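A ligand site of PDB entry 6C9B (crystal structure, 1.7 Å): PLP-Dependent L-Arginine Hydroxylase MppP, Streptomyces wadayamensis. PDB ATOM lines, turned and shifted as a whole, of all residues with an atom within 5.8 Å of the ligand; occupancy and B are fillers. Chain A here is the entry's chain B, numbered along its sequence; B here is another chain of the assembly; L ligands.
The side-chain hydroxyl of Ser 91 lies within hydrogen-bond range of a nitrogen (N3) of the ligand (3.1 Å). N2 of the ligand lies close to ND2 of Asn 117. An oxygen (O3) of the ligand is in hydrogen-bond range of the backbone NH (N) of Gly 28 (2.8 Å). The guanidinium group (NH1) of Arg 352 lies within salt-bridge range of an oxygen (O3) of the ligand. NE2 of His 29 sits at hydrogen-bond distance from O1 of the ligand (2.7 Å). The side-chain hydroxyl of Thr 12 is in hydrogen-bond range of a nitrogen (N1) of the ligand (2.9 Å). A nitrogen (N2) of the ligand is in hydrogen-bond range of the backbone carbonyl oxygen (O) of Ser 248 of chain B, at 2.9 Å. The backbone carbonyl oxygen (O) of Asp 249 of chain B sits at hydrogen-bond distance from a nitrogen (N2) of the ligand, 3.2 Å away. The side-chain carboxylate of Glu 15 lies close to an oxygen (O3) of the ligand. O of Ile 250 of chain B sits at hydrogen-bond distance from N3 of the ligand (3.3 Å). O1 of the ligand is in hydrogen-bond range of OP3 of LLP 221, at 2.6 Å. The side-chain amide nitrogen (ND2) of Asn 160 lies within hydrogen-bond range of an oxygen (O2) of the ligand, at 3.1 Å.
The side-chain hydroxyl (OG) of Ser 91 sits at hydrogen-bond distance from the side-chain amide nitrogen (ND2) of Asn 117 (2.6 Å). The backbone NH (N) of His 29 sits at hydrogen-bond distance from the side-chain carboxylate (OD1) of Asp 27 (3.1 Å). OP2 of LLP 221 is in salt-bridge range of the side-chain amino group of Lys 229 (2.7 Å). O of Leu 334 lies within hydrogen-bond range of N of Arg 352. O3 of LLP 221 is in hydrogen-bond range of ND2 of Asn 160, at 2.8 Å. OG of Ser 91 is in hydrogen-bond range of OP1 of LLP 221 (2.7 Å). The side-chain hydroxyl (OG) of Ser 91 lies close to the backbone carbonyl oxygen (O) of Ile 250 of chain B (3.5 Å). O of Asp 249 of chain B lies within hydrogen-bond range of ND2 of Asn 117, 2.9 Å away.
Asp 27 touches the ligand. CZ of Phe 115 touches O4 of the ligand (3.0 Å). CA of Leu 251 of chain B touches N3 of the ligand, at 3.8 Å. Leu 252 of chain B touches the ligand (CB to C2, 3.8 Å). Hydrophobic or aromatic side chains that line the ligand: His 29, Phe 115 and Leu 252 of chain B. Within 4 Å of the ligand: Thr 12, Glu 15, Asp 27, Gly 28, His 29, Ser 91, Phe 115, Asn 117, Asn 160, LLP 221, Arg 352, Ser 248 of chain B, Asp 249 of chain B, Ile 250 of chain B, Leu 251 of chain B and Leu 252 of chain B. The nearest printed residue that does not touch the ligand is Ala 26 (4.4 Å).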
ATOM      1  N   THR A  12     -29.244 -27.963  -0.858  1.00  0.00           N
ATOM      2  CA  THR A  12     -27.854 -28.147  -1.292  1.00  0.00           C
ATOM      3  C   THR A  12     -27.462 -29.619  -1.258  1.00  0.00           C
ATOM      4  O   THR A  12     -26.729 -30.090  -2.131  1.00  0.00           O
ATOM      5  CB  THR A  12     -26.942 -27.288  -0.420  1.00  0.00           C
ATOM      6  OG1 THR A  12     -27.320 -25.912  -0.581  1.00  0.00           O
ATOM      7  CG2 THR A  12     -25.447 -27.455  -0.785  1.00  0.00           C
ATOM      8  N   GLU A  15     -28.529 -31.136  -4.196  1.00  0.00           N
ATOM      9  CA  GLU A  15     -27.696 -30.718  -5.321  1.00  0.00           C
ATOM     10  C   GLU A  15     -26.365 -31.464  -5.361  1.00  0.00           C
ATOM     11  O   GLU A  15     -25.817 -31.645  -6.456  1.00  0.00           O
ATOM     12  CB  GLU A  15     -27.467 -29.197  -5.262  1.00  0.00           C
ATOM     13  CG  GLU A  15     -28.788 -28.416  -5.445  1.00  0.00           C
ATOM     14  CD  GLU A  15     -28.638 -26.895  -5.322  1.00  0.00           C
ATOM     15  OE1 GLU A  15     -27.591 -26.404  -4.855  1.00  0.00           O
ATOM     16  OE2 GLU A  15     -29.573 -26.190  -5.716  1.00  0.00           O
ATOM     17  N   ALA A  26     -30.236 -29.600 -11.577  1.00  0.00           N
ATOM     18  CA  ALA A  26     -30.573 -29.355 -10.184  1.00  0.00           C
ATOM     19  C   ALA A  26     -30.053 -27.999  -9.715  1.00  0.00           C
ATOM     20  O   ALA A  26     -30.848 -27.061  -9.544  1.00  0.00           O
ATOM     21  CB  ALA A  26     -30.015 -30.451  -9.279  1.00  0.00           C
ATOM     22  N   ASP A  27     -28.750 -27.871  -9.465  1.00  0.00           N
ATOM     23  CA  ASP A  27     -28.296 -26.625  -8.863  1.00  0.00           C
ATOM     24  C   ASP A  27     -28.437 -25.491  -9.873  1.00  0.00           C
ATOM     25  O   ASP A  27     -28.444 -25.684 -11.092  1.00  0.00           O
ATOM     26  CB  ASP A  27     -26.855 -26.719  -8.378  1.00  0.00           C
ATOM     27  CG  ASP A  27     -25.897 -26.897  -9.510  1.00  0.00           C
ATOM     28  OD1 ASP A  27     -25.730 -25.938 -10.307  1.00  0.00           O
ATOM     29  OD2 ASP A  27     -25.315 -27.997  -9.595  1.00  0.00           O
ATOM     30  N   GLY A  28     -28.543 -24.281  -9.337  1.00  0.00           N
ATOM     31  CA  GLY A  28     -28.865 -23.168 -10.190  1.00  0.00           C
ATOM     32  C   GLY A  28     -27.680 -22.480 -10.821  1.00  0.00           C
ATOM     33  O   GLY A  28     -27.889 -21.526 -11.574  1.00  0.00           O
ATOM     34  N   HIS A  29     -26.467 -22.948 -10.563  1.00  0.00           N
ATOM     35  CA  HIS A  29     -25.280 -22.329 -11.111  1.00  0.00           C
ATOM     36  C   HIS A  29     -25.304 -22.385 -12.632  1.00  0.00           C
ATOM     37  O   HIS A  29     -25.969 -23.215 -13.250  1.00  0.00           O
ATOM     38  CB  HIS A  29     -24.017 -23.023 -10.604  1.00  0.00           C
ATOM     39  CG  HIS A  29     -23.849 -22.928  -9.118  1.00  0.00           C
ATOM     40  ND1 HIS A  29     -22.632 -23.122  -8.496  1.00  0.00           N
ATOM     41  CD2 HIS A  29     -24.738 -22.671  -8.132  1.00  0.00           C
ATOM     42  CE1 HIS A  29     -22.787 -22.984  -7.193  1.00  0.00           C
ATOM     43  NE2 HIS A  29     -24.049 -22.697  -6.940  1.00  0.00           N
ATOM     44  N   SER A  91     -23.598 -16.499  -0.040  1.00  0.00           N
ATOM     45  CA  SER A  91     -23.868 -17.177   1.228  1.00  0.00           C
ATOM     46  C   SER A  91     -22.883 -16.771   2.333  1.00  0.00           C
ATOM     47  O   SER A  91     -23.266 -16.726   3.503  1.00  0.00           O
ATOM     48  CB  SER A  91     -23.822 -18.684   1.074  1.00  0.00           C
ATOM     49  OG  SER A  91     -24.860 -19.121   0.195  1.00  0.00           O
ATOM     50  N   PHE A 115     -34.854 -19.428  -1.351  1.00  0.00           N
ATOM     51  CA  PHE A 115     -33.720 -20.349  -1.320  1.00  0.00           C
ATOM     52  C   PHE A 115     -33.391 -20.688   0.136  1.00  0.00           C
ATOM     53  O   PHE A 115     -33.249 -19.793   0.977  1.00  0.00           O
ATOM     54  CB  PHE A 115     -32.529 -19.702  -2.035  1.00  0.00           C
ATOM     55  CG  PHE A 115     -31.258 -20.480  -1.915  1.00  0.00           C
ATOM     56  CD1 PHE A 115     -31.256 -21.874  -2.001  1.00  0.00           C
ATOM     57  CD2 PHE A 115     -30.047 -19.817  -1.722  1.00  0.00           C
ATOM     58  CE1 PHE A 115     -30.073 -22.588  -1.897  1.00  0.00           C
ATOM     59  CE2 PHE A 115     -28.863 -20.520  -1.627  1.00  0.00           C
ATOM     60  CZ  PHE A 115     -28.877 -21.919  -1.697  1.00  0.00           C
ATOM     61  N   ASN A 117     -31.093 -21.760   2.057  1.00  0.00           N
ATOM     62  CA  ASN A 117     -29.963 -21.521   2.932  1.00  0.00           C
ATOM     63  C   ASN A 117     -30.067 -20.150   3.597  1.00  0.00           C
ATOM     64  O   ASN A 117     -29.485 -19.966   4.673  1.00  0.00           O
ATOM     65  CB  ASN A 117     -28.636 -21.738   2.212  1.00  0.00           C
ATOM     66  CG  ASN A 117     -28.174 -20.573   1.452  1.00  0.00           C
ATOM     67  OD1 ASN A 117     -28.950 -19.722   1.029  1.00  0.00           O
ATOM     68  ND2 ASN A 117     -26.860 -20.511   1.233  1.00  0.00           N
ATOM     69  N   ASN A 160     -35.951 -16.603  -5.722  1.00  0.00           N
ATOM     70  CA  ASN A 160     -35.552 -17.971  -6.049  1.00  0.00           C
ATOM     71  C   ASN A 160     -36.397 -18.818  -5.120  1.00  0.00           C
ATOM     72  O   ASN A 160     -36.195 -18.760  -3.900  1.00  0.00           O
ATOM     73  CB  ASN A 160     -34.066 -18.167  -5.774  1.00  0.00           C
ATOM     74  CG  ASN A 160     -33.586 -19.538  -6.058  1.00  0.00           C
ATOM     75  OD1 ASN A 160     -34.345 -20.430  -6.443  1.00  0.00           O
ATOM     76  ND2 ASN A 160     -32.290 -19.717  -5.935  1.00  0.00           N
ATOM     77  N   PHE A 191     -30.475 -12.940  -8.450  1.00  0.00           N
ATOM     78  CA  PHE A 191     -31.078 -13.144  -9.762  1.00  0.00           C
ATOM     79  C   PHE A 191     -31.289 -11.831 -10.513  1.00  0.00           C
ATOM     80  O   PHE A 191     -31.920 -11.842 -11.571  1.00  0.00           O
ATOM     81  CB  PHE A 191     -32.407 -13.887  -9.635  1.00  0.00           C
ATOM     82  CG  PHE A 191     -32.309 -15.398  -9.448  1.00  0.00           C
ATOM     83  CD1 PHE A 191     -31.107 -16.059  -9.412  1.00  0.00           C
ATOM     84  CD2 PHE A 191     -33.489 -16.148  -9.368  1.00  0.00           C
ATOM     85  CE1 PHE A 191     -31.053 -17.460  -9.272  1.00  0.00           C
ATOM     86  CE2 PHE A 191     -33.452 -17.509  -9.224  1.00  0.00           C
ATOM     87  CZ  PHE A 191     -32.228 -18.180  -9.189  1.00  0.00           C
ATOM     88  N1  LLP A 221     -29.100 -16.186  -2.879  1.00  0.00           N
ATOM     89  C2  LLP A 221     -29.809 -16.653  -3.925  1.00  0.00           C
ATOM     90  C2' LLP A 221     -31.228 -16.160  -4.028  1.00  0.00           C
ATOM     91  C3  LLP A 221     -29.260 -17.558  -4.875  1.00  0.00           C
ATOM     92  O3  LLP A 221     -30.093 -17.937  -5.885  1.00  0.00           O
ATOM     93  C4  LLP A 221     -27.935 -17.994  -4.729  1.00  0.00           C
ATOM     94  C4' LLP A 221     -27.338 -18.901  -5.722  1.00  0.00           C
ATOM     95  C5  LLP A 221     -27.238 -17.481  -3.605  1.00  0.00           C
ATOM     96  C6  LLP A 221     -27.855 -16.609  -2.731  1.00  0.00           C
ATOM     97  C5' LLP A 221     -25.831 -17.699  -3.194  1.00  0.00           C
ATOM     98  OP4 LLP A 221     -25.261 -18.757  -3.750  1.00  0.00           O
ATOM     99  P   LLP A 221     -23.776 -19.230  -3.376  1.00  0.00           P
ATOM    100  OP1 LLP A 221     -23.389 -18.727  -2.033  1.00  0.00           O
ATOM    101  OP2 LLP A 221     -22.904 -18.799  -4.596  1.00  0.00           O
ATOM    102  OP3 LLP A 221     -24.043 -20.772  -3.462  1.00  0.00           O
ATOM    103  N   LLP A 221     -24.535 -16.320 -10.293  1.00  0.00           N
ATOM    104  CA  LLP A 221     -25.535 -17.079 -11.015  1.00  0.00           C
ATOM    105  CB  LLP A 221     -26.931 -16.900 -10.354  1.00  0.00           C
ATOM    106  CG  LLP A 221     -27.072 -17.588  -9.017  1.00  0.00           C
ATOM    107  CD  LLP A 221     -27.325 -19.067  -9.193  1.00  0.00           C
ATOM    108  CE  LLP A 221     -27.273 -19.844  -7.867  1.00  0.00           C
ATOM    109  NZ  LLP A 221     -27.964 -19.158  -6.811  1.00  0.00           N
ATOM    110  C   LLP A 221     -25.677 -16.726 -12.490  1.00  0.00           C
ATOM    111  O   LLP A 221     -26.241 -17.444 -13.302  1.00  0.00           O
ATOM    112  N   LYS A 229     -16.610 -16.073  -8.424  1.00  0.00           N
ATOM    113  CA  LYS A 229     -17.712 -15.151  -8.174  1.00  0.00           C
ATOM    114  C   LYS A 229     -17.400 -14.330  -6.927  1.00  0.00           C
ATOM    115  O   LYS A 229     -16.426 -14.577  -6.211  1.00  0.00           O
ATOM    116  CB  LYS A 229     -19.006 -15.937  -7.965  1.00  0.00           C
ATOM    117  CG  LYS A 229     -18.964 -16.800  -6.687  1.00  0.00           C
ATOM    118  CD  LYS A 229     -19.898 -17.979  -6.705  1.00  0.00           C
ATOM    119  CE  LYS A 229     -19.620 -18.862  -5.487  1.00  0.00           C
ATOM    120  NZ  LYS A 229     -20.633 -19.946  -5.428  1.00  0.00           N
ATOM    121  N   VAL A 309     -34.133 -20.513 -13.220  1.00  0.00           N
ATOM    122  CA  VAL A 309     -34.674 -21.761 -12.719  1.00  0.00           C
ATOM    123  C   VAL A 309     -36.176 -21.763 -12.990  1.00  0.00           C
ATOM    124  O   VAL A 309     -36.808 -20.718 -13.117  1.00  0.00           O
ATOM    125  CB  VAL A 309     -34.373 -21.959 -11.228  1.00  0.00           C
ATOM    126  CG1 VAL A 309     -32.864 -22.007 -10.994  1.00  0.00           C
ATOM    127  CG2 VAL A 309     -35.013 -20.828 -10.364  1.00  0.00           C
ATOM    128  N   LEU A 334     -34.508 -31.028  -8.732  1.00  0.00           N
ATOM    129  CA  LEU A 334     -34.557 -30.649  -7.323  1.00  0.00           C
ATOM    130  C   LEU A 334     -35.999 -30.666  -6.822  1.00  0.00           C
ATOM    131  O   LEU A 334     -36.846 -29.939  -7.364  1.00  0.00           O
ATOM    132  CB  LEU A 334     -33.937 -29.263  -7.177  1.00  0.00           C
ATOM    133  CG  LEU A 334     -33.427 -28.788  -5.830  1.00  0.00           C
ATOM    134  CD1 LEU A 334     -32.374 -29.734  -5.345  1.00  0.00           C
ATOM    135  CD2 LEU A 334     -32.878 -27.368  -6.013  1.00  0.00           C
ATOM    136  N   PHE A 339     -37.638 -25.306  -0.371  1.00  0.00           N
ATOM    137  CA  PHE A 339     -37.798 -23.861  -0.539  1.00  0.00           C
ATOM    138  C   PHE A 339     -38.901 -23.322   0.345  1.00  0.00           C
ATOM    139  O   PHE A 339     -38.918 -22.130   0.675  1.00  0.00           O
ATOM    140  CB  PHE A 339     -38.151 -23.516  -1.978  1.00  0.00           C
ATOM    141  CG  PHE A 339     -37.071 -23.827  -2.977  1.00  0.00           C
ATOM    142  CD1 PHE A 339     -36.012 -22.955  -3.180  1.00  0.00           C
ATOM    143  CD2 PHE A 339     -37.155 -24.968  -3.747  1.00  0.00           C
ATOM    144  CE1 PHE A 339     -35.028 -23.243  -4.110  1.00  0.00           C
ATOM    145  CE2 PHE A 339     -36.171 -25.256  -4.677  1.00  0.00           C
ATOM    146  CZ  PHE A 339     -35.114 -24.399  -4.855  1.00  0.00           C
ATOM    147  N   ARG A 352     -37.959 -28.380  -9.316  1.00  0.00           N
ATOM    148  CA  ARG A 352     -37.313 -27.228  -9.929  1.00  0.00           C
ATOM    149  C   ARG A 352     -36.273 -27.709 -10.924  1.00  0.00           C
ATOM    150  O   ARG A 352     -35.511 -28.640 -10.633  1.00  0.00           O
ATOM    151  CB  ARG A 352     -36.655 -26.322  -8.877  1.00  0.00           C
ATOM    152  CG  ARG A 352     -36.380 -24.920  -9.381  1.00  0.00           C
ATOM    153  CD  ARG A 352     -35.435 -24.136  -8.453  1.00  0.00           C
ATOM    154  NE  ARG A 352     -34.062 -24.665  -8.550  1.00  0.00           N
ATOM    155  CZ  ARG A 352     -32.993 -24.074  -8.018  1.00  0.00           C
ATOM    156  NH1 ARG A 352     -31.800 -24.628  -8.152  1.00  0.00           N
ATOM    157  NH2 ARG A 352     -33.104 -22.940  -7.341  1.00  0.00           N
ATOM    158  N   TYR B 247     -21.644 -26.749   6.756  1.00  0.00           N
ATOM    159  CA  TYR B 247     -20.948 -26.593   5.486  1.00  0.00           C
ATOM    160  C   TYR B 247     -21.935 -26.452   4.331  1.00  0.00           C
ATOM    161  O   TYR B 247     -21.818 -25.539   3.498  1.00  0.00           O
ATOM    162  CB  TYR B 247     -20.016 -27.794   5.269  1.00  0.00           C
ATOM    163  CG  TYR B 247     -19.352 -27.835   3.893  1.00  0.00           C
ATOM    164  CD1 TYR B 247     -20.000 -28.439   2.828  1.00  0.00           C
ATOM    165  CD2 TYR B 247     -18.117 -27.249   3.684  1.00  0.00           C
ATOM    166  CE1 TYR B 247     -19.424 -28.451   1.572  1.00  0.00           C
ATOM    167  CE2 TYR B 247     -17.517 -27.278   2.419  1.00  0.00           C
ATOM    168  CZ  TYR B 247     -18.196 -27.883   1.374  1.00  0.00           C
ATOM    169  OH  TYR B 247     -17.619 -27.895   0.118  1.00  0.00           O
ATOM    170  N   SER B 248     -22.917 -27.348   4.265  1.00  0.00           N
ATOM    171  CA  SER B 248     -23.880 -27.335   3.168  1.00  0.00           C
ATOM    172  C   SER B 248     -24.823 -26.118   3.226  1.00  0.00           C
ATOM    173  O   SER B 248     -25.368 -25.728   2.189  1.00  0.00           O
ATOM    174  CB  SER B 248     -24.656 -28.649   3.159  1.00  0.00           C
ATOM    175  OG  SER B 248     -25.600 -28.773   4.215  1.00  0.00           O
ATOM    176  N   ASP B 249     -25.013 -25.518   4.387  1.00  0.00           N
ATOM    177  CA  ASP B 249     -25.712 -24.234   4.457  1.00  0.00           C
ATOM    178  C   ASP B 249     -24.925 -23.106   3.809  1.00  0.00           C
ATOM    179  O   ASP B 249     -25.525 -22.143   3.284  1.00  0.00           O
ATOM    180  CB  ASP B 249     -25.985 -23.875   5.910  1.00  0.00           C
ATOM    181  CG  ASP B 249     -26.979 -24.812   6.625  1.00  0.00           C
ATOM    182  OD1 ASP B 249     -27.769 -25.524   5.979  1.00  0.00           O
ATOM    183  OD2 ASP B 249     -26.956 -24.802   7.881  1.00  0.00           O
ATOM    184  N   ILE B 250     -23.605 -23.206   3.805  1.00  0.00           N
ATOM    185  CA  ILE B 250     -22.774 -22.128   3.299  1.00  0.00           C
ATOM    186  C   ILE B 250     -22.388 -22.352   1.845  1.00  0.00           C
ATOM    187  O   ILE B 250     -22.390 -21.388   1.080  1.00  0.00           O
ATOM    188  CB  ILE B 250     -21.535 -21.945   4.188  1.00  0.00           C
ATOM    189  CG1 ILE B 250     -21.987 -21.474   5.582  1.00  0.00           C
ATOM    190  CG2 ILE B 250     -20.551 -20.948   3.578  1.00  0.00           C
ATOM    191  CD1 ILE B 250     -20.879 -21.298   6.559  1.00  0.00           C
ATOM    192  N   LEU B 251     -22.044 -23.563   1.417  1.00  0.00           N
ATOM    193  CA  LEU B 251     -21.608 -23.693   0.024  1.00  0.00           C
ATOM    194  C   LEU B 251     -21.828 -25.097  -0.537  1.00  0.00           C
ATOM    195  O   LEU B 251     -21.897 -26.104   0.185  1.00  0.00           O
ATOM    196  CB  LEU B 251     -20.137 -23.299  -0.142  1.00  0.00           C
ATOM    197  CG  LEU B 251     -19.069 -24.213   0.449  1.00  0.00           C
ATOM    198  CD1 LEU B 251     -17.728 -23.874  -0.167  1.00  0.00           C
ATOM    199  CD2 LEU B 251     -18.944 -24.076   1.972  1.00  0.00           C
ATOM    200  N   LEU B 252     -21.940 -25.131  -1.868  1.00  0.00           N
ATOM    201  CA  LEU B 252     -22.037 -26.344  -2.672  1.00  0.00           C
ATOM    202  C   LEU B 252     -20.658 -26.958  -2.894  1.00  0.00           C
ATOM    203  O   LEU B 252     -20.548 -28.158  -3.162  1.00  0.00           O
ATOM    204  CB  LEU B 252     -22.679 -25.997  -4.018  1.00  0.00           C
ATOM    205  CG  LEU B 252     -22.957 -27.094  -5.043  1.00  0.00           C
ATOM    206  CD1 LEU B 252     -23.943 -28.128  -4.521  1.00  0.00           C
ATOM    207  CD2 LEU B 252     -23.483 -26.445  -6.331  1.00  0.00           C
HETATM  208  C1  LIG L   1     -29.588 -22.801  -6.260  1.00  0.00           C
HETATM  209  C2  LIG L   1     -25.510 -23.497  -3.360  1.00  0.00           C
HETATM  210  C3  LIG L   1     -25.513 -23.076  -0.901  1.00  0.00           C
HETATM  211  C4  LIG L   1     -26.429 -22.475  -4.003  1.00  0.00           C
HETATM  212  C5  LIG L   1     -27.667 -23.236  -4.515  1.00  0.00           C
HETATM  213  C6  LIG L   1     -28.791 -22.310  -5.060  1.00  0.00           C
HETATM  214  N1  LIG L   1     -25.922 -23.869  -2.018  1.00  0.00           N
HETATM  215  N2  LIG L   1     -25.907 -23.444   0.402  1.00  0.00           N
HETATM  216  N3  LIG L   1     -24.792 -21.989  -1.092  1.00  0.00           N
HETATM  217  O1  LIG L   1     -25.795 -21.870  -5.055  1.00  0.00           O
HETATM  218  O2  LIG L   1     -30.344 -21.997  -6.771  1.00  0.00           O
HETATM  219  O3  LIG L   1     -29.475 -23.956  -6.696  1.00  0.00           O
HETATM  220  O4  LIG L   1     -29.036 -21.210  -4.562  1.00  0.00           O
